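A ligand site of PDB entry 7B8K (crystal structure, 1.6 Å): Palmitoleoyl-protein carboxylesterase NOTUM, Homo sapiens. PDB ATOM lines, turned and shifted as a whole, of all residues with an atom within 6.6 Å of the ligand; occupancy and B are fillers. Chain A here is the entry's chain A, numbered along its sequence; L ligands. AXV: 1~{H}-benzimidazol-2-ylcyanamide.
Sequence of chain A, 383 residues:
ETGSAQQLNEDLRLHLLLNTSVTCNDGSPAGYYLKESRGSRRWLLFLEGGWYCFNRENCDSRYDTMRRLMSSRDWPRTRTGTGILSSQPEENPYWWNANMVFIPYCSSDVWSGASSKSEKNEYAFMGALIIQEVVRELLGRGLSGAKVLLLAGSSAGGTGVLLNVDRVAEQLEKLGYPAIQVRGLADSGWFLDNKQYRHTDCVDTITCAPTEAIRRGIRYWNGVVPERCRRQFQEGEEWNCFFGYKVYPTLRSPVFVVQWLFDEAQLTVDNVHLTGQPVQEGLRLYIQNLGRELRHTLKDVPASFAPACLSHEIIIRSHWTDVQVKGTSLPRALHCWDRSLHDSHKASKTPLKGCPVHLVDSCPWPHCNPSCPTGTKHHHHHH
OG1 of Thr 159 is in hydrogen-bond range of N2 of the ligand (2.9 Å).
N3 of the ligand lies close to N of Ala 156 (3.4 Å).
CA of Trp 51 touches N4 of the ligand, at 3.3 Å.
Tyr 52 touches the ligand (CE2 to N1, 3.9 Å).
C of Ser 155 touches N3 of the ligand, at 3.8 Å.
Phe 191 touches the ligand.
Ile 214 touches the ligand.
Phe 242 touches the ligand.
Phe 243 touches the ligand.
Within 4 Å of the ligand: Trp 51, Tyr 52, Ser 155, Ala 156, Thr 159, Phe 191, Ile 214, Phe 242 and Phe 243.
The nearest printed residue that does not touch the ligand is Pro 210 (4.1 Å).
OH of Tyr 105 sits at hydrogen-bond distance from O of Trp 51.
The side-chain hydroxyl (OG) of Ser 155 is in hydrogen-bond range of a ring nitrogen (NE2) of His 312, at 3.1 Å.
The side-chain hydroxyl (OG1) of Thr 159 sits at hydrogen-bond distance from the backbone carbonyl oxygen (O) of Gly 189 (3.0 Å).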
ATOM      1  N   GLY A  49     -28.431 -23.140 -34.857  1.00  0.00           N
ATOM      2  CA  GLY A  49     -28.573 -23.775 -33.565  1.00  0.00           C
ATOM      3  C   GLY A  49     -29.903 -24.488 -33.402  1.00  0.00           C
ATOM      4  O   GLY A  49     -30.666 -24.653 -34.361  1.00  0.00           O
ATOM      5  N   GLY A  50     -30.161 -24.941 -32.164  1.00  0.00           N
ATOM      6  CA  GLY A  50     -31.425 -25.586 -31.835  1.00  0.00           C
ATOM      7  C   GLY A  50     -31.339 -26.781 -30.899  1.00  0.00           C
ATOM      8  O   GLY A  50     -31.853 -27.859 -31.231  1.00  0.00           O
ATOM      9  N   TRP A  51     -30.726 -26.610 -29.728  1.00  0.00           N
ATOM     10  CA  TRP A  51     -30.610 -27.662 -28.691  1.00  0.00           C
ATOM     11  C   TRP A  51     -29.907 -28.905 -29.260  1.00  0.00           C
ATOM     12  O   TRP A  51     -28.977 -28.775 -30.084  1.00  0.00           O
ATOM     13  CB  TRP A  51     -31.967 -27.925 -28.059  1.00  0.00           C
ATOM     14  CG  TRP A  51     -32.436 -26.783 -27.210  1.00  0.00           C
ATOM     15  CD1 TRP A  51     -33.317 -25.797 -27.572  1.00  0.00           C
ATOM     16  CD2 TRP A  51     -32.016 -26.463 -25.875  1.00  0.00           C
ATOM     17  NE1 TRP A  51     -33.492 -24.914 -26.539  1.00  0.00           N
ATOM     18  CE2 TRP A  51     -32.699 -25.291 -25.485  1.00  0.00           C
ATOM     19  CE3 TRP A  51     -31.120 -27.061 -24.975  1.00  0.00           C
ATOM     20  CZ2 TRP A  51     -32.525 -24.714 -24.230  1.00  0.00           C
ATOM     21  CZ3 TRP A  51     -30.954 -26.479 -23.723  1.00  0.00           C
ATOM     22  CH2 TRP A  51     -31.660 -25.316 -23.362  1.00  0.00           C
ATOM     23  N   TYR A  52     -30.304 -30.098 -28.801  1.00  0.00           N
ATOM     24  CA  TYR A  52     -29.657 -31.374 -29.139  1.00  0.00           C
ATOM     25  C   TYR A  52     -30.533 -32.494 -28.586  1.00  0.00           C
ATOM     26  O   TYR A  52     -31.526 -32.236 -27.904  1.00  0.00           O
ATOM     27  CB  TYR A  52     -28.249 -31.504 -28.548  1.00  0.00           C
ATOM     28  CG  TYR A  52     -28.144 -31.051 -27.102  1.00  0.00           C
ATOM     29  CD1 TYR A  52     -28.451 -31.922 -26.058  1.00  0.00           C
ATOM     30  CD2 TYR A  52     -27.751 -29.754 -26.775  1.00  0.00           C
ATOM     31  CE1 TYR A  52     -28.367 -31.506 -24.729  1.00  0.00           C
ATOM     32  CE2 TYR A  52     -27.660 -29.336 -25.459  1.00  0.00           C
ATOM     33  CZ  TYR A  52     -27.976 -30.217 -24.444  1.00  0.00           C
ATOM     34  OH  TYR A  52     -27.885 -29.799 -23.128  1.00  0.00           O
ATOM     35  N   TYR A 105     -28.825 -27.039 -39.284  1.00  0.00           N
ATOM     36  CA  TYR A 105     -28.461 -27.929 -38.179  1.00  0.00           C
ATOM     37  C   TYR A 105     -29.413 -29.120 -38.218  1.00  0.00           C
ATOM     38  O   TYR A 105     -30.575 -29.021 -37.818  1.00  0.00           O
ATOM     39  CB  TYR A 105     -28.543 -27.168 -36.858  1.00  0.00           C
ATOM     40  CG  TYR A 105     -28.236 -27.914 -35.568  1.00  0.00           C
ATOM     41  CD1 TYR A 105     -27.112 -28.733 -35.441  1.00  0.00           C
ATOM     42  CD2 TYR A 105     -28.987 -27.663 -34.417  1.00  0.00           C
ATOM     43  CE1 TYR A 105     -26.798 -29.369 -34.215  1.00  0.00           C
ATOM     44  CE2 TYR A 105     -28.681 -28.286 -33.210  1.00  0.00           C
ATOM     45  CZ  TYR A 105     -27.594 -29.132 -33.112  1.00  0.00           C
ATOM     46  OH  TYR A 105     -27.310 -29.744 -31.899  1.00  0.00           O
ATOM     47  N   VAL A 110     -24.603 -30.766 -31.354  1.00  0.00           N
ATOM     48  CA  VAL A 110     -23.870 -29.522 -31.071  1.00  0.00           C
ATOM     49  C   VAL A 110     -22.686 -29.463 -32.062  1.00  0.00           C
ATOM     50  O   VAL A 110     -21.622 -28.884 -31.775  1.00  0.00           O
ATOM     51  CB  VAL A 110     -23.433 -29.459 -29.586  1.00  0.00           C
ATOM     52  CG1 VAL A 110     -22.648 -28.183 -29.241  1.00  0.00           C
ATOM     53  CG2 VAL A 110     -24.583 -29.775 -28.620  1.00  0.00           C
ATOM     54  N   SER A 155     -26.211 -20.150 -30.676  1.00  0.00           N
ATOM     55  CA  SER A 155     -26.652 -21.153 -29.688  1.00  0.00           C
ATOM     56  C   SER A 155     -25.825 -22.423 -29.865  1.00  0.00           C
ATOM     57  O   SER A 155     -24.599 -22.354 -29.717  1.00  0.00           O
ATOM     58  CB  SER A 155     -28.169 -21.372 -29.782  1.00  0.00           C
ATOM     59  OG  SER A 155     -28.859 -20.150 -29.828  1.00  0.00           O
ATOM     60  N   ALA A 156     -26.446 -23.585 -30.133  1.00  0.00           N
ATOM     61  CA  ALA A 156     -25.655 -24.782 -30.408  1.00  0.00           C
ATOM     62  C   ALA A 156     -24.654 -24.553 -31.537  1.00  0.00           C
ATOM     63  O   ALA A 156     -23.559 -25.143 -31.519  1.00  0.00           O
ATOM     64  CB  ALA A 156     -26.576 -25.969 -30.740  1.00  0.00           C
ATOM     65  N   GLY A 157     -24.981 -23.680 -32.507  1.00  0.00           N
ATOM     66  CA  GLY A 157     -24.020 -23.355 -33.550  1.00  0.00           C
ATOM     67  C   GLY A 157     -22.868 -22.483 -33.080  1.00  0.00           C
ATOM     68  O   GLY A 157     -21.767 -22.552 -33.633  1.00  0.00           O
ATOM     69  N   THR A 159     -21.525 -22.832 -29.982  1.00  0.00           N
ATOM     70  CA  THR A 159     -20.625 -23.840 -29.422  1.00  0.00           C
ATOM     71  C   THR A 159     -19.935 -24.611 -30.544  1.00  0.00           C
ATOM     72  O   THR A 159     -18.736 -24.927 -30.448  1.00  0.00           O
ATOM     73  CB  THR A 159     -21.396 -24.795 -28.483  1.00  0.00           C
ATOM     74  OG1 THR A 159     -22.147 -24.027 -27.541  1.00  0.00           O
ATOM     75  CG2 THR A 159     -20.444 -25.721 -27.730  1.00  0.00           C
ATOM     76  N   SER A 188     -23.939 -16.727 -28.407  1.00  0.00           N
ATOM     77  CA  SER A 188     -24.808 -17.487 -27.473  1.00  0.00           C
ATOM     78  C   SER A 188     -24.387 -18.940 -27.316  1.00  0.00           C
ATOM     79  O   SER A 188     -25.231 -19.813 -27.046  1.00  0.00           O
ATOM     80  CB  SER A 188     -26.293 -17.419 -27.840  1.00  0.00           C
ATOM     81  OG  SER A 188     -26.779 -16.095 -27.733  1.00  0.00           O
ATOM     82  N   GLY A 189     -23.095 -19.225 -27.416  1.00  0.00           N
ATOM     83  CA  GLY A 189     -22.612 -20.569 -27.232  1.00  0.00           C
ATOM     84  C   GLY A 189     -21.608 -20.734 -26.092  1.00  0.00           C
ATOM     85  O   GLY A 189     -20.902 -21.748 -26.042  1.00  0.00           O
ATOM     86  N   TRP A 190     -21.547 -19.746 -25.200  1.00  0.00           N
ATOM     87  CA  TRP A 190     -20.567 -19.680 -24.112  1.00  0.00           C
ATOM     88  C   TRP A 190     -21.292 -19.949 -22.787  1.00  0.00           C
ATOM     89  O   TRP A 190     -21.782 -19.022 -22.136  1.00  0.00           O
ATOM     90  CB  TRP A 190     -19.902 -18.287 -24.156  1.00  0.00           C
ATOM     91  CG  TRP A 190     -18.761 -17.995 -23.218  1.00  0.00           C
ATOM     92  CD1 TRP A 190     -18.834 -17.552 -21.909  1.00  0.00           C
ATOM     93  CD2 TRP A 190     -17.355 -18.037 -23.546  1.00  0.00           C
ATOM     94  NE1 TRP A 190     -17.555 -17.351 -21.412  1.00  0.00           N
ATOM     95  CE2 TRP A 190     -16.636 -17.636 -22.387  1.00  0.00           C
ATOM     96  CE3 TRP A 190     -16.637 -18.386 -24.707  1.00  0.00           C
ATOM     97  CZ2 TRP A 190     -15.240 -17.571 -22.360  1.00  0.00           C
ATOM     98  CZ3 TRP A 190     -15.233 -18.333 -24.662  1.00  0.00           C
ATOM     99  CH2 TRP A 190     -14.556 -17.922 -23.507  1.00  0.00           C
ATOM    100  N   PHE A 191     -21.343 -21.227 -22.387  1.00  0.00           N
ATOM    101  CA  PHE A 191     -22.102 -21.674 -21.223  1.00  0.00           C
ATOM    102  C   PHE A 191     -21.204 -21.895 -19.998  1.00  0.00           C
ATOM    103  O   PHE A 191     -19.985 -22.106 -20.104  1.00  0.00           O
ATOM    104  CB  PHE A 191     -22.861 -22.993 -21.520  1.00  0.00           C
ATOM    105  CG  PHE A 191     -24.070 -22.848 -22.431  1.00  0.00           C
ATOM    106  CD1 PHE A 191     -23.919 -22.674 -23.814  1.00  0.00           C
ATOM    107  CD2 PHE A 191     -25.347 -22.913 -21.907  1.00  0.00           C
ATOM    108  CE1 PHE A 191     -25.045 -22.551 -24.646  1.00  0.00           C
ATOM    109  CE2 PHE A 191     -26.478 -22.787 -22.718  1.00  0.00           C
ATOM    110  CZ  PHE A 191     -26.313 -22.613 -24.101  1.00  0.00           C
ATOM    111  N   LEU A 192     -21.839 -21.906 -18.817  1.00  0.00           N
ATOM    112  CA  LEU A 192     -21.158 -22.181 -17.562  1.00  0.00           C
ATOM    113  C   LEU A 192     -21.671 -23.494 -16.959  1.00  0.00           C
ATOM    114  O   LEU A 192     -22.883 -23.760 -16.970  1.00  0.00           O
ATOM    115  CB  LEU A 192     -21.392 -21.047 -16.557  1.00  0.00           C
ATOM    116  CG  LEU A 192     -20.948 -19.632 -16.962  1.00  0.00           C
ATOM    117  CD1 LEU A 192     -21.378 -18.638 -15.878  1.00  0.00           C
ATOM    118  CD2 LEU A 192     -19.450 -19.556 -17.225  1.00  0.00           C
ATOM    119  N   PRO A 210     -26.467 -29.876 -17.538  1.00  0.00           N
ATOM    120  CA  PRO A 210     -25.661 -29.702 -18.754  1.00  0.00           C
ATOM    121  C   PRO A 210     -24.426 -30.595 -18.809  1.00  0.00           C
ATOM    122  O   PRO A 210     -24.196 -31.222 -19.844  1.00  0.00           O
ATOM    123  CB  PRO A 210     -25.261 -28.231 -18.691  1.00  0.00           C
ATOM    124  CG  PRO A 210     -26.432 -27.589 -18.075  1.00  0.00           C
ATOM    125  CD  PRO A 210     -26.890 -28.566 -16.998  1.00  0.00           C
ATOM    126  N   THR A 211     -23.649 -30.651 -17.722  1.00  0.00           N
ATOM    127  CA  THR A 211     -22.469 -31.503 -17.730  1.00  0.00           C
ATOM    128  C   THR A 211     -22.854 -32.956 -17.988  1.00  0.00           C
ATOM    129  O   THR A 211     -22.248 -33.633 -18.826  1.00  0.00           O
ATOM    130  CB  THR A 211     -21.697 -31.377 -16.413  1.00  0.00           C
ATOM    131  OG1 THR A 211     -22.516 -31.846 -15.338  1.00  0.00           O
ATOM    132  CG2 THR A 211     -21.298 -29.940 -16.157  1.00  0.00           C
ATOM    133  N   ILE A 214     -24.156 -33.347 -21.688  1.00  0.00           N
ATOM    134  CA  ILE A 214     -23.044 -33.392 -22.638  1.00  0.00           C
ATOM    135  C   ILE A 214     -22.252 -34.686 -22.487  1.00  0.00           C
ATOM    136  O   ILE A 214     -21.813 -35.295 -23.472  1.00  0.00           O
ATOM    137  CB  ILE A 214     -22.134 -32.156 -22.474  1.00  0.00           C
ATOM    138  CG1 ILE A 214     -22.909 -30.849 -22.703  1.00  0.00           C
ATOM    139  CG2 ILE A 214     -20.934 -32.248 -23.401  1.00  0.00           C
ATOM    140  CD1 ILE A 214     -23.550 -30.749 -24.066  1.00  0.00           C
ATOM    141  N   TRP A 239     -16.020 -33.820 -22.275  1.00  0.00           N
ATOM    142  CA  TRP A 239     -17.156 -32.911 -22.105  1.00  0.00           C
ATOM    143  C   TRP A 239     -16.715 -31.526 -21.659  1.00  0.00           C
ATOM    144  O   TRP A 239     -17.418 -30.536 -21.892  1.00  0.00           O
ATOM    145  CB  TRP A 239     -18.168 -33.484 -21.088  1.00  0.00           C
ATOM    146  CG  TRP A 239     -17.630 -33.616 -19.668  1.00  0.00           C
ATOM    147  CD1 TRP A 239     -17.101 -34.732 -19.098  1.00  0.00           C
ATOM    148  CD2 TRP A 239     -17.577 -32.579 -18.665  1.00  0.00           C
ATOM    149  NE1 TRP A 239     -16.717 -34.462 -17.802  1.00  0.00           N
ATOM    150  CE2 TRP A 239     -16.992 -33.149 -17.513  1.00  0.00           C
ATOM    151  CE3 TRP A 239     -17.954 -31.240 -18.630  1.00  0.00           C
ATOM    152  CZ2 TRP A 239     -16.785 -32.420 -16.337  1.00  0.00           C
ATOM    153  CZ3 TRP A 239     -17.747 -30.516 -17.463  1.00  0.00           C
ATOM    154  CH2 TRP A 239     -17.164 -31.102 -16.336  1.00  0.00           C
ATOM    155  N   PHE A 242     -16.700 -28.636 -24.285  1.00  0.00           N
ATOM    156  CA  PHE A 242     -17.891 -27.954 -24.768  1.00  0.00           C
ATOM    157  C   PHE A 242     -18.182 -26.646 -24.035  1.00  0.00           C
ATOM    158  O   PHE A 242     -19.112 -25.933 -24.410  1.00  0.00           O
ATOM    159  CB  PHE A 242     -19.141 -28.846 -24.655  1.00  0.00           C
ATOM    160  CG  PHE A 242     -19.235 -29.958 -25.671  1.00  0.00           C
ATOM    161  CD1 PHE A 242     -18.250 -30.927 -25.786  1.00  0.00           C
ATOM    162  CD2 PHE A 242     -20.354 -30.061 -26.499  1.00  0.00           C
ATOM    163  CE1 PHE A 242     -18.369 -31.955 -26.711  1.00  0.00           C
ATOM    164  CE2 PHE A 242     -20.480 -31.083 -27.426  1.00  0.00           C
ATOM    165  CZ  PHE A 242     -19.488 -32.036 -27.529  1.00  0.00           C
ATOM    166  N   PHE A 243     -17.399 -26.302 -23.008  1.00  0.00           N
ATOM    167  CA  PHE A 243     -17.613 -25.083 -22.239  1.00  0.00           C
ATOM    168  C   PHE A 243     -16.578 -24.047 -22.658  1.00  0.00           C
ATOM    169  O   PHE A 243     -15.378 -24.271 -22.488  1.00  0.00           O
ATOM    170  CB  PHE A 243     -17.555 -25.372 -20.740  1.00  0.00           C
ATOM    171  CG  PHE A 243     -18.735 -26.173 -20.266  1.00  0.00           C
ATOM    172  CD1 PHE A 243     -18.737 -27.560 -20.384  1.00  0.00           C
ATOM    173  CD2 PHE A 243     -19.888 -25.540 -19.808  1.00  0.00           C
ATOM    174  CE1 PHE A 243     -19.833 -28.304 -20.005  1.00  0.00           C
ATOM    175  CE2 PHE A 243     -20.997 -26.296 -19.421  1.00  0.00           C
ATOM    176  CZ  PHE A 243     -20.970 -27.672 -19.523  1.00  0.00           C
ATOM    177  N   GLY A 244     -17.070 -22.920 -23.201  1.00  0.00           N
ATOM    178  CA  GLY A 244     -16.209 -21.922 -23.822  1.00  0.00           C
ATOM    179  C   GLY A 244     -15.001 -21.503 -22.996  1.00  0.00           C
ATOM    180  O   GLY A 244     -13.887 -21.436 -23.514  1.00  0.00           O
ATOM    181  N   ALA A 265     -31.101 -19.581 -22.377  1.00  0.00           N
ATOM    182  CA  ALA A 265     -30.789 -21.013 -22.366  1.00  0.00           C
ATOM    183  C   ALA A 265     -30.005 -21.391 -21.103  1.00  0.00           C
ATOM    184  O   ALA A 265     -30.256 -22.442 -20.502  1.00  0.00           O
ATOM    185  CB  ALA A 265     -30.013 -21.392 -23.628  1.00  0.00           C
ATOM    186  N   VAL A 269     -31.359 -24.189 -18.309  1.00  0.00           N
ATOM    187  CA  VAL A 269     -30.661 -25.351 -17.778  1.00  0.00           C
ATOM    188  C   VAL A 269     -30.320 -25.173 -16.298  1.00  0.00           C
ATOM    189  O   VAL A 269     -30.071 -26.174 -15.609  1.00  0.00           O
ATOM    190  CB  VAL A 269     -29.392 -25.658 -18.606  1.00  0.00           C
ATOM    191  CG1 VAL A 269     -29.761 -26.032 -20.040  1.00  0.00           C
ATOM    192  CG2 VAL A 269     -28.412 -24.499 -18.596  1.00  0.00           C
ATOM    193  N   HIS A 312     -31.652 -14.255 -26.132  1.00  0.00           N
ATOM    194  CA  HIS A 312     -31.113 -15.485 -26.702  1.00  0.00           C
ATOM    195  C   HIS A 312     -30.828 -15.281 -28.189  1.00  0.00           C
ATOM    196  O   HIS A 312     -31.755 -15.004 -28.947  1.00  0.00           O
ATOM    197  CB  HIS A 312     -32.101 -16.640 -26.493  1.00  0.00           C
ATOM    198  CG  HIS A 312     -31.571 -17.970 -26.911  1.00  0.00           C
ATOM    199  ND1 HIS A 312     -32.143 -18.717 -27.921  1.00  0.00           N
ATOM    200  CD2 HIS A 312     -30.528 -18.699 -26.451  1.00  0.00           C
ATOM    201  CE1 HIS A 312     -31.466 -19.853 -28.065  1.00  0.00           C
ATOM    202  NE2 HIS A 312     -30.483 -19.857 -27.180  1.00  0.00           N
HETATM  203  N1  AXV L   1     -25.807 -25.990 -24.841  1.00  0.00           N
HETATM  204  N3  AXV L   1     -26.088 -25.047 -27.106  1.00  0.00           N
HETATM  205  C4  AXV L   1     -23.608 -25.990 -24.708  1.00  0.00           C
HETATM  206  C5  AXV L   1     -24.754 -26.311 -24.017  1.00  0.00           C
HETATM  207  C6  AXV L   1     -24.643 -26.855 -22.709  1.00  0.00           C
HETATM  208  C7  AXV L   1     -25.316 -25.507 -25.968  1.00  0.00           C
HETATM  209  C8  AXV L   1     -27.520 -25.305 -27.122  1.00  0.00           C
HETATM  210  C1  AXV L   1     -23.390 -27.061 -22.147  1.00  0.00           C
HETATM  211  C2  AXV L   1     -22.231 -26.732 -22.854  1.00  0.00           C
HETATM  212  C3  AXV L   1     -22.326 -26.203 -24.132  1.00  0.00           C
HETATM  213  N2  AXV L   1     -23.989 -25.502 -25.926  1.00  0.00           N
HETATM  214  N4  AXV L   1     -28.628 -25.510 -27.139  1.00  0.00           N
